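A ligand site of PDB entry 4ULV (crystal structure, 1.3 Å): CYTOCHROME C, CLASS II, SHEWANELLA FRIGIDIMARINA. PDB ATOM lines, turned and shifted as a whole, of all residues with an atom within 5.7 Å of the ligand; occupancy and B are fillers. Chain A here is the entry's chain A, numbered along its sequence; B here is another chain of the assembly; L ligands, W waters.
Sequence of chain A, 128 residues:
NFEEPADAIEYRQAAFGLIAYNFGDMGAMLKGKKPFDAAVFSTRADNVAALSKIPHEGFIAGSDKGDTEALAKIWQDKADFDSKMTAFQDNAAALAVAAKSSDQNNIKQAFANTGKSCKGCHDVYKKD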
ATOM      1  N   ILE A   9      -0.711  15.399   8.324  1.00  0.00           N
ATOM      2  CA  ILE A   9      -1.656  16.162   9.123  1.00  0.00           C
ATOM      3  C   ILE A   9      -2.187  17.357   8.390  1.00  0.00           C
ATOM      4  O   ILE A   9      -3.416  17.592   8.357  1.00  0.00           O
ATOM      5  CB  ILE A   9      -0.943  16.670  10.423  1.00  0.00           C
ATOM      6  CG1 ILE A   9      -0.596  15.493  11.308  1.00  0.00           C
ATOM      7  CG2 ILE A   9      -1.800  17.693  11.123  1.00  0.00           C
ATOM      8  CD1 ILE A   9       0.524  15.805  12.375  1.00  0.00           C
ATOM      9  N   ARG A  12      -4.832  16.042   5.780  1.00  0.00           N
ATOM     10  CA  ARG A  12      -6.198  15.689   6.286  1.00  0.00           C
ATOM     11  C   ARG A  12      -6.948  16.934   6.781  1.00  0.00           C
ATOM     12  O   ARG A  12      -8.140  17.055   6.590  1.00  0.00           O
ATOM     13  CB  ARG A  12      -6.148  14.572   7.321  1.00  0.00           C
ATOM     14  CG  ARG A  12      -5.583  14.959   8.685  1.00  0.00           C
ATOM     15  CD  ARG A  12      -4.849  13.806   9.278  1.00  0.00           C
ATOM     16  NE  ARG A  12      -4.465  14.061  10.681  1.00  0.00           N
ATOM     17  CZ  ARG A  12      -3.582  13.318  11.340  1.00  0.00           C
ATOM     18  NH1 ARG A  12      -2.921  12.333  10.748  1.00  0.00           N
ATOM     19  NH2 ARG A  12      -3.354  13.528  12.642  1.00  0.00           N
ATOM     20  N   GLN A  13      -6.246  17.841   7.471  1.00  0.00           N
ATOM     21  CA  GLN A  13      -6.863  19.107   7.922  1.00  0.00           C
ATOM     22  C   GLN A  13      -7.423  19.990   6.778  1.00  0.00           C
ATOM     23  O   GLN A  13      -8.532  20.514   6.843  1.00  0.00           O
ATOM     24  CB  GLN A  13      -5.911  19.942   8.791  1.00  0.00           C
ATOM     25  CG  GLN A  13      -5.570  19.247  10.101  1.00  0.00           C
ATOM     26  CD  GLN A  13      -4.506  19.993  10.907  1.00  0.00           C
ATOM     27  OE1 GLN A  13      -3.703  20.751  10.341  1.00  0.00           O
ATOM     28  NE2 GLN A  13      -4.497  19.746  12.208  1.00  0.00           N
ATOM     29  N   ALA A  14      -6.648  20.056   5.697  1.00  0.00           N
ATOM     30  CA  ALA A  14      -7.044  20.820   4.513  1.00  0.00           C
ATOM     31  C   ALA A  14      -8.355  20.219   3.943  1.00  0.00           C
ATOM     32  O   ALA A  14      -9.280  20.960   3.652  1.00  0.00           O
ATOM     33  CB  ALA A  14      -5.983  20.786   3.441  1.00  0.00           C
ATOM     34  N   PHE A  16     -10.633  18.321   5.512  1.00  0.00           N
ATOM     35  CA  PHE A  16     -11.745  18.592   6.439  1.00  0.00           C
ATOM     36  C   PHE A  16     -12.237  20.012   6.377  1.00  0.00           C
ATOM     37  O   PHE A  16     -13.445  20.257   6.463  1.00  0.00           O
ATOM     38  CB  PHE A  16     -11.425  18.185   7.869  1.00  0.00           C
ATOM     39  CG  PHE A  16     -11.422  16.685   8.112  1.00  0.00           C
ATOM     40  CD1 PHE A  16     -12.560  15.902   7.899  1.00  0.00           C
ATOM     41  CD2 PHE A  16     -10.288  16.091   8.627  1.00  0.00           C
ATOM     42  CE1 PHE A  16     -12.498  14.552   8.194  1.00  0.00           C
ATOM     43  CE2 PHE A  16     -10.238  14.776   8.904  1.00  0.00           C
ATOM     44  CZ  PHE A  16     -11.330  13.989   8.656  1.00  0.00           C
ATOM     45  N   GLY A  17     -11.334  20.969   6.231  1.00  0.00           N
ATOM     46  CA  GLY A  17     -11.798  22.305   6.054  1.00  0.00           C
ATOM     47  C   GLY A  17     -12.698  22.524   4.858  1.00  0.00           C
ATOM     48  O   GLY A  17     -13.641  23.287   4.874  1.00  0.00           O
ATOM     49  N   ILE A  19     -14.416  20.194   3.355  1.00  0.00           N
ATOM     50  CA  ILE A  19     -15.696  19.472   3.654  1.00  0.00           C
ATOM     51  C   ILE A  19     -16.583  20.423   4.441  1.00  0.00           C
ATOM     52  O   ILE A  19     -17.802  20.584   4.162  1.00  0.00           O
ATOM     53  CB  ILE A  19     -15.425  18.191   4.407  1.00  0.00           C
ATOM     54  CG1 ILE A  19     -14.783  17.157   3.502  1.00  0.00           C
ATOM     55  CG2 ILE A  19     -16.669  17.640   5.090  1.00  0.00           C
ATOM     56  CD1 ILE A  19     -14.218  15.975   4.214  1.00  0.00           C
ATOM     57  N   ALA A  20     -16.003  21.030   5.493  1.00  0.00           N
ATOM     58  CA  ALA A  20     -16.810  21.898   6.431  1.00  0.00           C
ATOM     59  C   ALA A  20     -17.396  23.085   5.672  1.00  0.00           C
ATOM     60  O   ALA A  20     -18.543  23.498   5.890  1.00  0.00           O
ATOM     61  CB  ALA A  20     -16.007  22.359   7.602  1.00  0.00           C
ATOM     62  N   PHE A  23     -20.285  21.598   3.433  1.00  0.00           N
ATOM     63  CA  PHE A  23     -21.372  21.083   4.266  1.00  0.00           C
ATOM     64  C   PHE A  23     -22.068  22.215   5.010  1.00  0.00           C
ATOM     65  O   PHE A  23     -23.300  22.210   5.218  1.00  0.00           O
ATOM     66  CB  PHE A  23     -20.801  20.065   5.254  1.00  0.00           C
ATOM     67  CG  PHE A  23     -21.851  19.251   5.982  1.00  0.00           C
ATOM     68  CD1 PHE A  23     -22.574  18.307   5.302  1.00  0.00           C
ATOM     69  CD2 PHE A  23     -22.040  19.358   7.325  1.00  0.00           C
ATOM     70  CE1 PHE A  23     -23.546  17.547   5.905  1.00  0.00           C
ATOM     71  CE2 PHE A  23     -22.988  18.613   7.964  1.00  0.00           C
ATOM     72  CZ  PHE A  23     -23.737  17.667   7.252  1.00  0.00           C
ATOM     73  N   VAL A  48     -18.939  17.358  -1.222  1.00  0.00           N
ATOM     74  CA  VAL A  48     -18.756  16.614   0.024  1.00  0.00           C
ATOM     75  C   VAL A  48     -18.528  15.113  -0.181  1.00  0.00           C
ATOM     76  O   VAL A  48     -17.714  14.455   0.438  1.00  0.00           O
ATOM     77  CB  VAL A  48     -19.935  16.902   1.049  1.00  0.00           C
ATOM     78  CG1 VAL A  48     -19.818  16.024   2.280  1.00  0.00           C
ATOM     79  CG2 VAL A  48     -19.926  18.383   1.429  1.00  0.00           C
ATOM     80  N   PHE A  59      -4.129   9.716   7.894  1.00  0.00           N
ATOM     81  CA  PHE A  59      -4.052   9.168   9.248  1.00  0.00           C
ATOM     82  C   PHE A  59      -3.005   8.074   9.435  1.00  0.00           C
ATOM     83  O   PHE A  59      -3.299   6.919   9.788  1.00  0.00           O
ATOM     84  CB  PHE A  59      -5.427   8.735   9.718  1.00  0.00           C
ATOM     85  CG  PHE A  59      -6.336   9.908  10.013  1.00  0.00           C
ATOM     86  CD1 PHE A  59      -6.308  10.542  11.263  1.00  0.00           C
ATOM     87  CD2 PHE A  59      -7.176  10.443   9.008  1.00  0.00           C
ATOM     88  CE1 PHE A  59      -7.108  11.625  11.473  1.00  0.00           C
ATOM     89  CE2 PHE A  59      -7.967  11.537   9.279  1.00  0.00           C
ATOM     90  CZ  PHE A  59      -7.929  12.127  10.529  1.00  0.00           C
ATOM     91  N   ASP A  67       1.056  19.089  15.275  1.00  0.00           N
ATOM     92  CA  ASP A  67       0.047  20.098  15.449  1.00  0.00           C
ATOM     93  C   ASP A  67      -1.302  19.525  14.936  1.00  0.00           C
ATOM     94  O   ASP A  67      -1.679  19.844  13.806  1.00  0.00           O
ATOM     95  CB  ASP A  67       0.401  21.388  14.701  1.00  0.00           C
ATOM     96  CG  ASP A  67      -0.635  22.459  14.923  1.00  0.00           C
ATOM     97  OD1 ASP A  67      -1.504  22.254  15.791  1.00  0.00           O
ATOM     98  OD2 ASP A  67      -0.643  23.451  14.168  1.00  0.00           O
ATOM     99  N   THR A  68      -1.984  18.775  15.807  1.00  0.00           N
ATOM    100  CA  THR A  68      -3.140  17.952  15.344  1.00  0.00           C
ATOM    101  C   THR A  68      -4.136  17.863  16.500  1.00  0.00           C
ATOM    102  O   THR A  68      -3.743  17.868  17.660  1.00  0.00           O
ATOM    103  CB  THR A  68      -2.663  16.567  14.843  1.00  0.00           C
ATOM    104  OG1 THR A  68      -3.814  15.841  14.362  1.00  0.00           O
ATOM    105  CG2 THR A  68      -2.058  15.690  15.900  1.00  0.00           C
ATOM    106  N   GLU A  69      -5.415  17.694  16.118  1.00  0.00           N
ATOM    107  CA  GLU A  69      -6.485  17.398  17.026  1.00  0.00           C
ATOM    108  C   GLU A  69      -6.901  15.956  16.963  1.00  0.00           C
ATOM    109  O   GLU A  69      -7.887  15.587  17.630  1.00  0.00           O
ATOM    110  CB  GLU A  69      -7.695  18.290  16.732  1.00  0.00           C
ATOM    111  CG  GLU A  69      -7.395  19.784  16.697  1.00  0.00           C
ATOM    112  CD  GLU A  69      -6.838  20.275  17.972  1.00  0.00           C
ATOM    113  OE1 GLU A  69      -7.530  20.141  19.027  1.00  0.00           O
ATOM    114  OE2 GLU A  69      -5.694  20.814  17.883  1.00  0.00           O
ATOM    115  N   ALA A  70      -6.179  15.146  16.193  1.00  0.00           N
ATOM    116  CA  ALA A  70      -6.420  13.721  16.187  1.00  0.00           C
ATOM    117  C   ALA A  70      -5.967  13.051  17.452  1.00  0.00           C
ATOM    118  O   ALA A  70      -4.874  13.306  17.893  1.00  0.00           O
ATOM    119  CB  ALA A  70      -5.769  13.117  14.972  1.00  0.00           C
ATOM    120  N   LEU A  71      -6.792  12.210  18.076  1.00  0.00           N
ATOM    121  CA  LEU A  71      -6.407  11.485  19.251  1.00  0.00           C
ATOM    122  C   LEU A  71      -5.654  10.217  18.962  1.00  0.00           C
ATOM    123  O   LEU A  71      -5.947   9.541  17.959  1.00  0.00           O
ATOM    124  CB  LEU A  71      -7.663  11.155  20.077  1.00  0.00           C
ATOM    125  CG  LEU A  71      -8.400  12.310  20.800  1.00  0.00           C
ATOM    126  CD1 LEU A  71      -9.746  11.907  21.400  1.00  0.00           C
ATOM    127  CD2 LEU A  71      -7.541  12.930  21.905  1.00  0.00           C
ATOM    128  N   ILE A  74      -7.305   6.809  17.665  1.00  0.00           N
ATOM    129  CA  ILE A  74      -7.516   6.393  16.268  1.00  0.00           C
ATOM    130  C   ILE A  74      -6.726   5.138  15.912  1.00  0.00           C
ATOM    131  O   ILE A  74      -7.217   4.241  15.245  1.00  0.00           O
ATOM    132  CB  ILE A  74      -7.148   7.562  15.344  1.00  0.00           C
ATOM    133  CG1 ILE A  74      -8.123   8.707  15.534  1.00  0.00           C
ATOM    134  CG2 ILE A  74      -6.987   7.106  13.883  1.00  0.00           C
ATOM    135  CD1 ILE A  74      -7.779   9.971  14.812  1.00  0.00           C
ATOM    136  N   PHE A  81     -12.355   3.288  13.549  1.00  0.00           N
ATOM    137  CA  PHE A  81     -12.170   4.508  12.818  1.00  0.00           C
ATOM    138  C   PHE A  81     -12.497   4.372  11.313  1.00  0.00           C
ATOM    139  O   PHE A  81     -13.154   5.235  10.721  1.00  0.00           O
ATOM    140  CB  PHE A  81     -10.717   5.033  13.008  1.00  0.00           C
ATOM    141  CG  PHE A  81     -10.468   6.358  12.351  1.00  0.00           C
ATOM    142  CD1 PHE A  81     -10.786   7.525  12.991  1.00  0.00           C
ATOM    143  CD2 PHE A  81      -9.812   6.443  11.110  1.00  0.00           C
ATOM    144  CE1 PHE A  81     -10.523   8.752  12.454  1.00  0.00           C
ATOM    145  CE2 PHE A  81      -9.521   7.677  10.567  1.00  0.00           C
ATOM    146  CZ  PHE A  81      -9.843   8.843  11.230  1.00  0.00           C
ATOM    147  N   LYS A  84     -16.186   3.930  10.678  1.00  0.00           N
ATOM    148  CA  LYS A  84     -16.841   5.267  10.696  1.00  0.00           C
ATOM    149  C   LYS A  84     -16.520   6.048   9.405  1.00  0.00           C
ATOM    150  O   LYS A  84     -17.365   6.740   8.827  1.00  0.00           O
ATOM    151  CB  LYS A  84     -16.423   6.099  11.925  1.00  0.00           C
ATOM    152  CG  LYS A  84     -17.024   5.617  13.203  1.00  0.00           C
ATOM    153  CD  LYS A  84     -16.707   6.601  14.359  1.00  0.00           C
ATOM    154  CE  LYS A  84     -17.105   6.151  15.753  1.00  0.00           C
ATOM    155  NZ  LYS A  84     -18.455   5.579  15.818  1.00  0.00           N
ATOM    156  N   MET A  85     -15.246   6.031   9.012  1.00  0.00           N
ATOM    157  CA  MET A  85     -14.882   6.784   7.799  1.00  0.00           C
ATOM    158  C   MET A  85     -15.578   6.279   6.542  1.00  0.00           C
ATOM    159  O   MET A  85     -16.043   7.095   5.756  1.00  0.00           O
ATOM    160  CB  MET A  85     -13.374   6.809   7.639  1.00  0.00           C
ATOM    161  CG  MET A  85     -12.907   7.737   6.519  1.00  0.00           C
ATOM    162  SD  MET A  85     -13.083   9.469   6.937  1.00  0.00           S
ATOM    163  CE  MET A  85     -11.759   9.749   8.154  1.00  0.00           C
ATOM    164  N   PHE A  88     -19.059   7.284   6.620  1.00  0.00           N
ATOM    165  CA  PHE A  88     -19.204   8.679   6.216  1.00  0.00           C
ATOM    166  C   PHE A  88     -19.193   8.831   4.692  1.00  0.00           C
ATOM    167  O   PHE A  88     -19.965   9.572   4.117  1.00  0.00           O
ATOM    168  CB  PHE A  88     -18.078   9.522   6.921  1.00  0.00           C
ATOM    169  CG  PHE A  88     -17.891  10.897   6.378  1.00  0.00           C
ATOM    170  CD1 PHE A  88     -18.959  11.766   6.200  1.00  0.00           C
ATOM    171  CD2 PHE A  88     -16.586  11.399   6.160  1.00  0.00           C
ATOM    172  CE1 PHE A  88     -18.767  13.063   5.755  1.00  0.00           C
ATOM    173  CE2 PHE A  88     -16.409  12.689   5.687  1.00  0.00           C
ATOM    174  CZ  PHE A  88     -17.465  13.542   5.493  1.00  0.00           C
ATOM    175  N   THR A 114     -25.668  12.593   7.659  1.00  0.00           N
ATOM    176  CA  THR A 114     -24.255  12.923   7.423  1.00  0.00           C
ATOM    177  C   THR A 114     -23.699  13.689   8.642  1.00  0.00           C
ATOM    178  O   THR A 114     -22.580  13.367   9.127  1.00  0.00           O
ATOM    179  CB  THR A 114     -24.168  13.696   6.152  1.00  0.00           C
ATOM    180  OG1 THR A 114     -24.652  12.890   5.040  1.00  0.00           O
ATOM    181  CG2 THR A 114     -22.741  14.084   5.838  1.00  0.00           C
ATOM    182  N   GLY A 115     -24.442  14.665   9.177  1.00  0.00           N
ATOM    183  CA  GLY A 115     -24.040  15.406  10.330  1.00  0.00           C
ATOM    184  C   GLY A 115     -23.744  14.523  11.506  1.00  0.00           C
ATOM    185  O   GLY A 115     -22.772  14.762  12.271  1.00  0.00           O
ATOM    186  N   SER A 117     -22.626  11.561  11.489  1.00  0.00           N
ATOM    187  CA  SER A 117     -21.366  10.866  11.357  1.00  0.00           C
ATOM    188  C   SER A 117     -20.185  11.774  11.670  1.00  0.00           C
ATOM    189  O   SER A 117     -19.239  11.279  12.249  1.00  0.00           O
ATOM    190  CB  SER A 117     -21.175  10.265   9.982  1.00  0.00           C
ATOM    191  OG  SER A 117     -21.166  11.271   9.014  1.00  0.00           O
ATOM    192  N   CYS A 118     -20.273  13.048  11.316  1.00  0.00           N
ATOM    193  CA  CYS A 118     -19.234  13.992  11.745  1.00  0.00           C
ATOM    194  C   CYS A 118     -19.094  13.980  13.240  1.00  0.00           C
ATOM    195  O   CYS A 118     -18.001  13.776  13.790  1.00  0.00           O
ATOM    196  CB  CYS A 118     -19.501  15.438  11.313  1.00  0.00           C
ATOM    197  SG  CYS A 118     -20.249  15.799   9.723  1.00  0.00           S
ATOM    198  N   CYS A 121     -17.819  10.625  14.899  1.00  0.00           N
ATOM    199  CA  CYS A 121     -16.428  10.486  14.857  1.00  0.00           C
ATOM    200  C   CYS A 121     -15.660  11.430  15.716  1.00  0.00           C
ATOM    201  O   CYS A 121     -14.746  11.005  16.475  1.00  0.00           O
ATOM    202  CB  CYS A 121     -15.942  10.534  13.398  1.00  0.00           C
ATOM    203  SG  CYS A 121     -14.173  10.077  13.316  1.00  0.00           S
ATOM    204  N   HIS A 122     -16.030  12.704  15.678  1.00  0.00           N
ATOM    205  CA  HIS A 122     -15.342  13.676  16.528  1.00  0.00           C
ATOM    206  C   HIS A 122     -15.450  13.324  18.018  1.00  0.00           C
ATOM    207  O   HIS A 122     -14.464  13.488  18.765  1.00  0.00           O
ATOM    208  CB  HIS A 122     -15.870  15.048  16.279  1.00  0.00           C
ATOM    209  CG  HIS A 122     -15.635  15.580  14.899  1.00  0.00           C
ATOM    210  ND1 HIS A 122     -16.186  16.755  14.462  1.00  0.00           N
ATOM    211  CD2 HIS A 122     -14.846  15.136  13.885  1.00  0.00           C
ATOM    212  CE1 HIS A 122     -15.744  17.012  13.236  1.00  0.00           C
ATOM    213  NE2 HIS A 122     -14.916  16.051  12.880  1.00  0.00           N
ATOM    214  N   TYR A 125     -12.764  10.454  18.438  1.00  0.00           N
ATOM    215  CA  TYR A 125     -11.421  10.485  17.866  1.00  0.00           C
ATOM    216  C   TYR A 125     -10.800  11.851  17.716  1.00  0.00           C
ATOM    217  O   TYR A 125      -9.631  11.920  17.262  1.00  0.00           O
ATOM    218  CB  TYR A 125     -11.475   9.755  16.533  1.00  0.00           C
ATOM    219  CG  TYR A 125     -11.753   8.302  16.681  1.00  0.00           C
ATOM    220  CD1 TYR A 125     -10.909   7.449  17.333  1.00  0.00           C
ATOM    221  CD2 TYR A 125     -12.903   7.737  16.125  1.00  0.00           C
ATOM    222  CE1 TYR A 125     -11.166   6.125  17.468  1.00  0.00           C
ATOM    223  CE2 TYR A 125     -13.176   6.400  16.268  1.00  0.00           C
ATOM    224  CZ  TYR A 125     -12.351   5.579  16.973  1.00  0.00           C
ATOM    225  OH  TYR A 125     -12.584   4.242  17.158  1.00  0.00           O
ATOM    226  N   LYS A 126     -11.454  12.916  18.118  1.00  0.00           N
ATOM    227  CA  LYS A 126     -10.938  14.281  17.965  1.00  0.00           C
ATOM    228  C   LYS A 126     -10.953  14.940  19.295  1.00  0.00           C
ATOM    229  O   LYS A 126     -11.848  14.803  20.106  1.00  0.00           O
ATOM    230  CB  LYS A 126     -11.765  15.125  16.963  1.00  0.00           C
ATOM    231  CG  LYS A 126     -11.169  16.436  16.516  1.00  0.00           C
ATOM    232  CD  LYS A 126     -12.058  17.180  15.561  1.00  0.00           C
ATOM    233  CE  LYS A 126     -11.619  18.556  15.136  1.00  0.00           C
ATOM    234  NZ  LYS A 126     -11.748  19.539  16.257  1.00  0.00           N
ATOM    235  N   GLU B  10      -7.266  30.750   2.214  1.00  0.00           N
ATOM    236  CA  GLU B  10      -7.023  29.458   2.804  1.00  0.00           C
ATOM    237  C   GLU B  10      -7.761  28.332   2.051  1.00  0.00           C
ATOM    238  O   GLU B  10      -7.209  27.234   1.834  1.00  0.00           O
ATOM    239  CB  GLU B  10      -7.463  29.489   4.274  1.00  0.00           C
ATOM    240  CG  GLU B  10      -7.258  28.211   5.008  1.00  0.00           C
ATOM    241  CD  GLU B  10      -7.748  28.263   6.459  1.00  0.00           C
ATOM    242  OE1 GLU B  10      -7.766  29.338   7.182  1.00  0.00           O
ATOM    243  OE2 GLU B  10      -8.085  27.162   6.923  1.00  0.00           O
HETATM  244 FE1  LIG L   1     -13.885  15.890  10.980  1.00  0.00          FE
HETATM  245  C1  LIG L   1     -11.040  17.598  11.867  1.00  0.00           C
HETATM  246  C2  LIG L   1     -15.246  18.783   9.893  1.00  0.00           C
HETATM  247  C3  LIG L   1     -16.391  14.133   9.527  1.00  0.00           C
HETATM  248  C4  LIG L   1     -12.435  12.994  11.983  1.00  0.00           C
HETATM  249  N1  LIG L   1     -13.206  17.873  10.883  1.00  0.00           N
HETATM  250  C5  LIG L   1     -12.041  18.401  11.310  1.00  0.00           C
HETATM  251  C6  LIG L   1     -11.998  19.787  11.113  1.00  0.00           C
HETATM  252  C7  LIG L   1     -13.195  20.119  10.560  1.00  0.00           C
HETATM  253  C8  LIG L   1     -13.929  18.904  10.411  1.00  0.00           C
HETATM  254  C9  LIG L   1     -13.662  21.483  10.186  1.00  0.00           C
HETATM  255  C10 LIG L   1     -10.829  20.710  11.487  1.00  0.00           C
HETATM  256  C11 LIG L   1      -9.838  20.798  10.310  1.00  0.00           C
HETATM  257  C12 LIG L   1      -8.692  21.776  10.577  1.00  0.00           C
HETATM  258  O1  LIG L   1      -7.795  21.429  11.342  1.00  0.00           O
HETATM  259  O2  LIG L   1      -8.702  22.849   9.961  1.00  0.00           O
HETATM  260  N2  LIG L   1     -15.508  16.353   9.788  1.00  0.00           N
HETATM  261  C13 LIG L   1     -15.996  17.601   9.545  1.00  0.00           C
HETATM  262  C14 LIG L   1     -17.286  17.615   8.999  1.00  0.00           C
HETATM  263  C15 LIG L   1     -17.563  16.273   8.906  1.00  0.00           C
HETATM  264  C16 LIG L   1     -16.504  15.520   9.387  1.00  0.00           C
HETATM  265  C17 LIG L   1     -18.139  18.776   8.706  1.00  0.00           C
HETATM  266  C18 LIG L   1     -18.826  15.600   8.394  1.00  0.00           C
HETATM  267  C19 LIG L   1     -19.476  16.270   7.188  1.00  0.00           C
HETATM  268  N3  LIG L   1     -14.334  13.864  10.708  1.00  0.00           N
HETATM  269  C20 LIG L   1     -15.477  13.309  10.147  1.00  0.00           C
HETATM  270  C21 LIG L   1     -15.476  11.906  10.281  1.00  0.00           C
HETATM  271  C22 LIG L   1     -14.312  11.565  10.977  1.00  0.00           C
HETATM  272  C23 LIG L   1     -13.666  12.834  11.218  1.00  0.00           C
HETATM  273  C24 LIG L   1     -16.595  11.009   9.765  1.00  0.00           C
HETATM  274  C25 LIG L   1     -13.823  10.238  11.455  1.00  0.00           C
HETATM  275  C26 LIG L   1     -14.225   8.986  10.721  1.00  0.00           C
HETATM  276  N4  LIG L   1     -12.025  15.367  11.767  1.00  0.00           N
HETATM  277  C27 LIG L   1     -11.664  14.176  12.227  1.00  0.00           C
HETATM  278  C28 LIG L   1     -10.434  14.208  12.946  1.00  0.00           C
HETATM  279  C29 LIG L   1     -10.001  15.499  12.817  1.00  0.00           C
HETATM  280  C30 LIG L   1     -11.026  16.210  12.140  1.00  0.00           C
HETATM  281  C31 LIG L   1      -9.722  13.091  13.579  1.00  0.00           C
HETATM  282  C32 LIG L   1      -8.687  16.051  13.287  1.00  0.00           C
HETATM  283  C33 LIG L   1      -7.655  16.193  12.168  1.00  0.00           C
HETATM  284  C34 LIG L   1      -6.311  16.761  12.651  1.00  0.00           C
HETATM  285  O3  LIG L   1      -6.363  17.745  13.471  1.00  0.00           O
HETATM  286  O4  LIG L   1      -5.300  16.157  12.261  1.00  0.00           O
HETATM  287  O   HOH W   1      -5.779  22.656  13.194  1.00  0.00           O
HETATM  288  O   HOH W   2     -10.963  23.979   9.108  1.00  0.00           O
HETATM  289  O   HOH W   3      -8.248  19.616  13.376  1.00  0.00           O
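The guanidinium group of Arg 12 lies within hydrogen-bond range of the side-chain hydroxyl of Thr 68.
OG1 of Thr 68 sits at hydrogen-bond distance from N of Ala 70 (3.1 Å).
The side-chain amide nitrogen of Gln 13 is in hydrogen-bond range of the backbone carbonyl oxygen of Asp 67, 3.2 Å away.
The backbone carbonyl oxygen of Thr 114 sits at hydrogen-bond distance from the side-chain hydroxyl of Ser 117 (2.5 Å).
The backbone carbonyl oxygen (O) of Tyr 125 lies within hydrogen-bond range of the backbone NH (N) of Leu 71 (3.0 Å).
CG2 of Ile 9 touches O4 of the ligand (3.99 Å).
Phe 16 touches the ligand.
Ile 19 touches the ligand (CG2 to C19, 3.8 Å).
Ala 20 touches the ligand.
Phe 23 touches the ligand (CG to C19, 3.998 Å).
Phe 59 touches the ligand (CE1 to C31, 3.7 Å).
Ala 70 touches the ligand (N to O3, 3.8 Å).
Ile 74 touches the ligand.
Phe 81 touches the ligand.
Lys 84 touches the ligand (CB to C26, 3.8 Å).
Met 85 touches the ligand (N to C26, 3.6 Å).
CB of Phe 88 touches C24 of the ligand, at 3.5 Å.
O of Ser 117 touches C24 of the ligand, at 3.6 Å.
Tyr 125 touches the ligand.
Lys 126 touches the ligand (CE to C1, 3.5 Å).
Hydrophobic or aromatic side chains that line the ligand: Ile 9, Phe 16, Ile 19, Ala 20, Phe 23, Phe 59, Ile 74, Phe 81, Met 85, Phe 88 and His 122.
Water W1 bridges an oxygen (O1) of the ligand (3.0 Å) and the side-chain amide nitrogen (NE2) of Gln 13 (3.3 Å).
The side-chain sulfur (SG) of Cys 121 is covalently linked to a carbon (C25) of the ligand (1.9 Å).
SG of Cys 118 is bonded to C18 of the ligand, 2.0 Å away.
NE2 of His 122 is bound to FE1 of the ligand, 2.2 Å away.
The side-chain hydroxyl of Thr 68 is in hydrogen-bond range of an oxygen (O4) of the ligand (2.6 Å).
An oxygen (O4) of the ligand lies within salt-bridge range of the guanidinium group of Arg 12 (2.8 Å).
N of Glu 69 sits at hydrogen-bond distance from O3 of the ligand.
NE2 of Gln 13 sits at hydrogen-bond distance from O3 of the ligand (3.0 Å).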
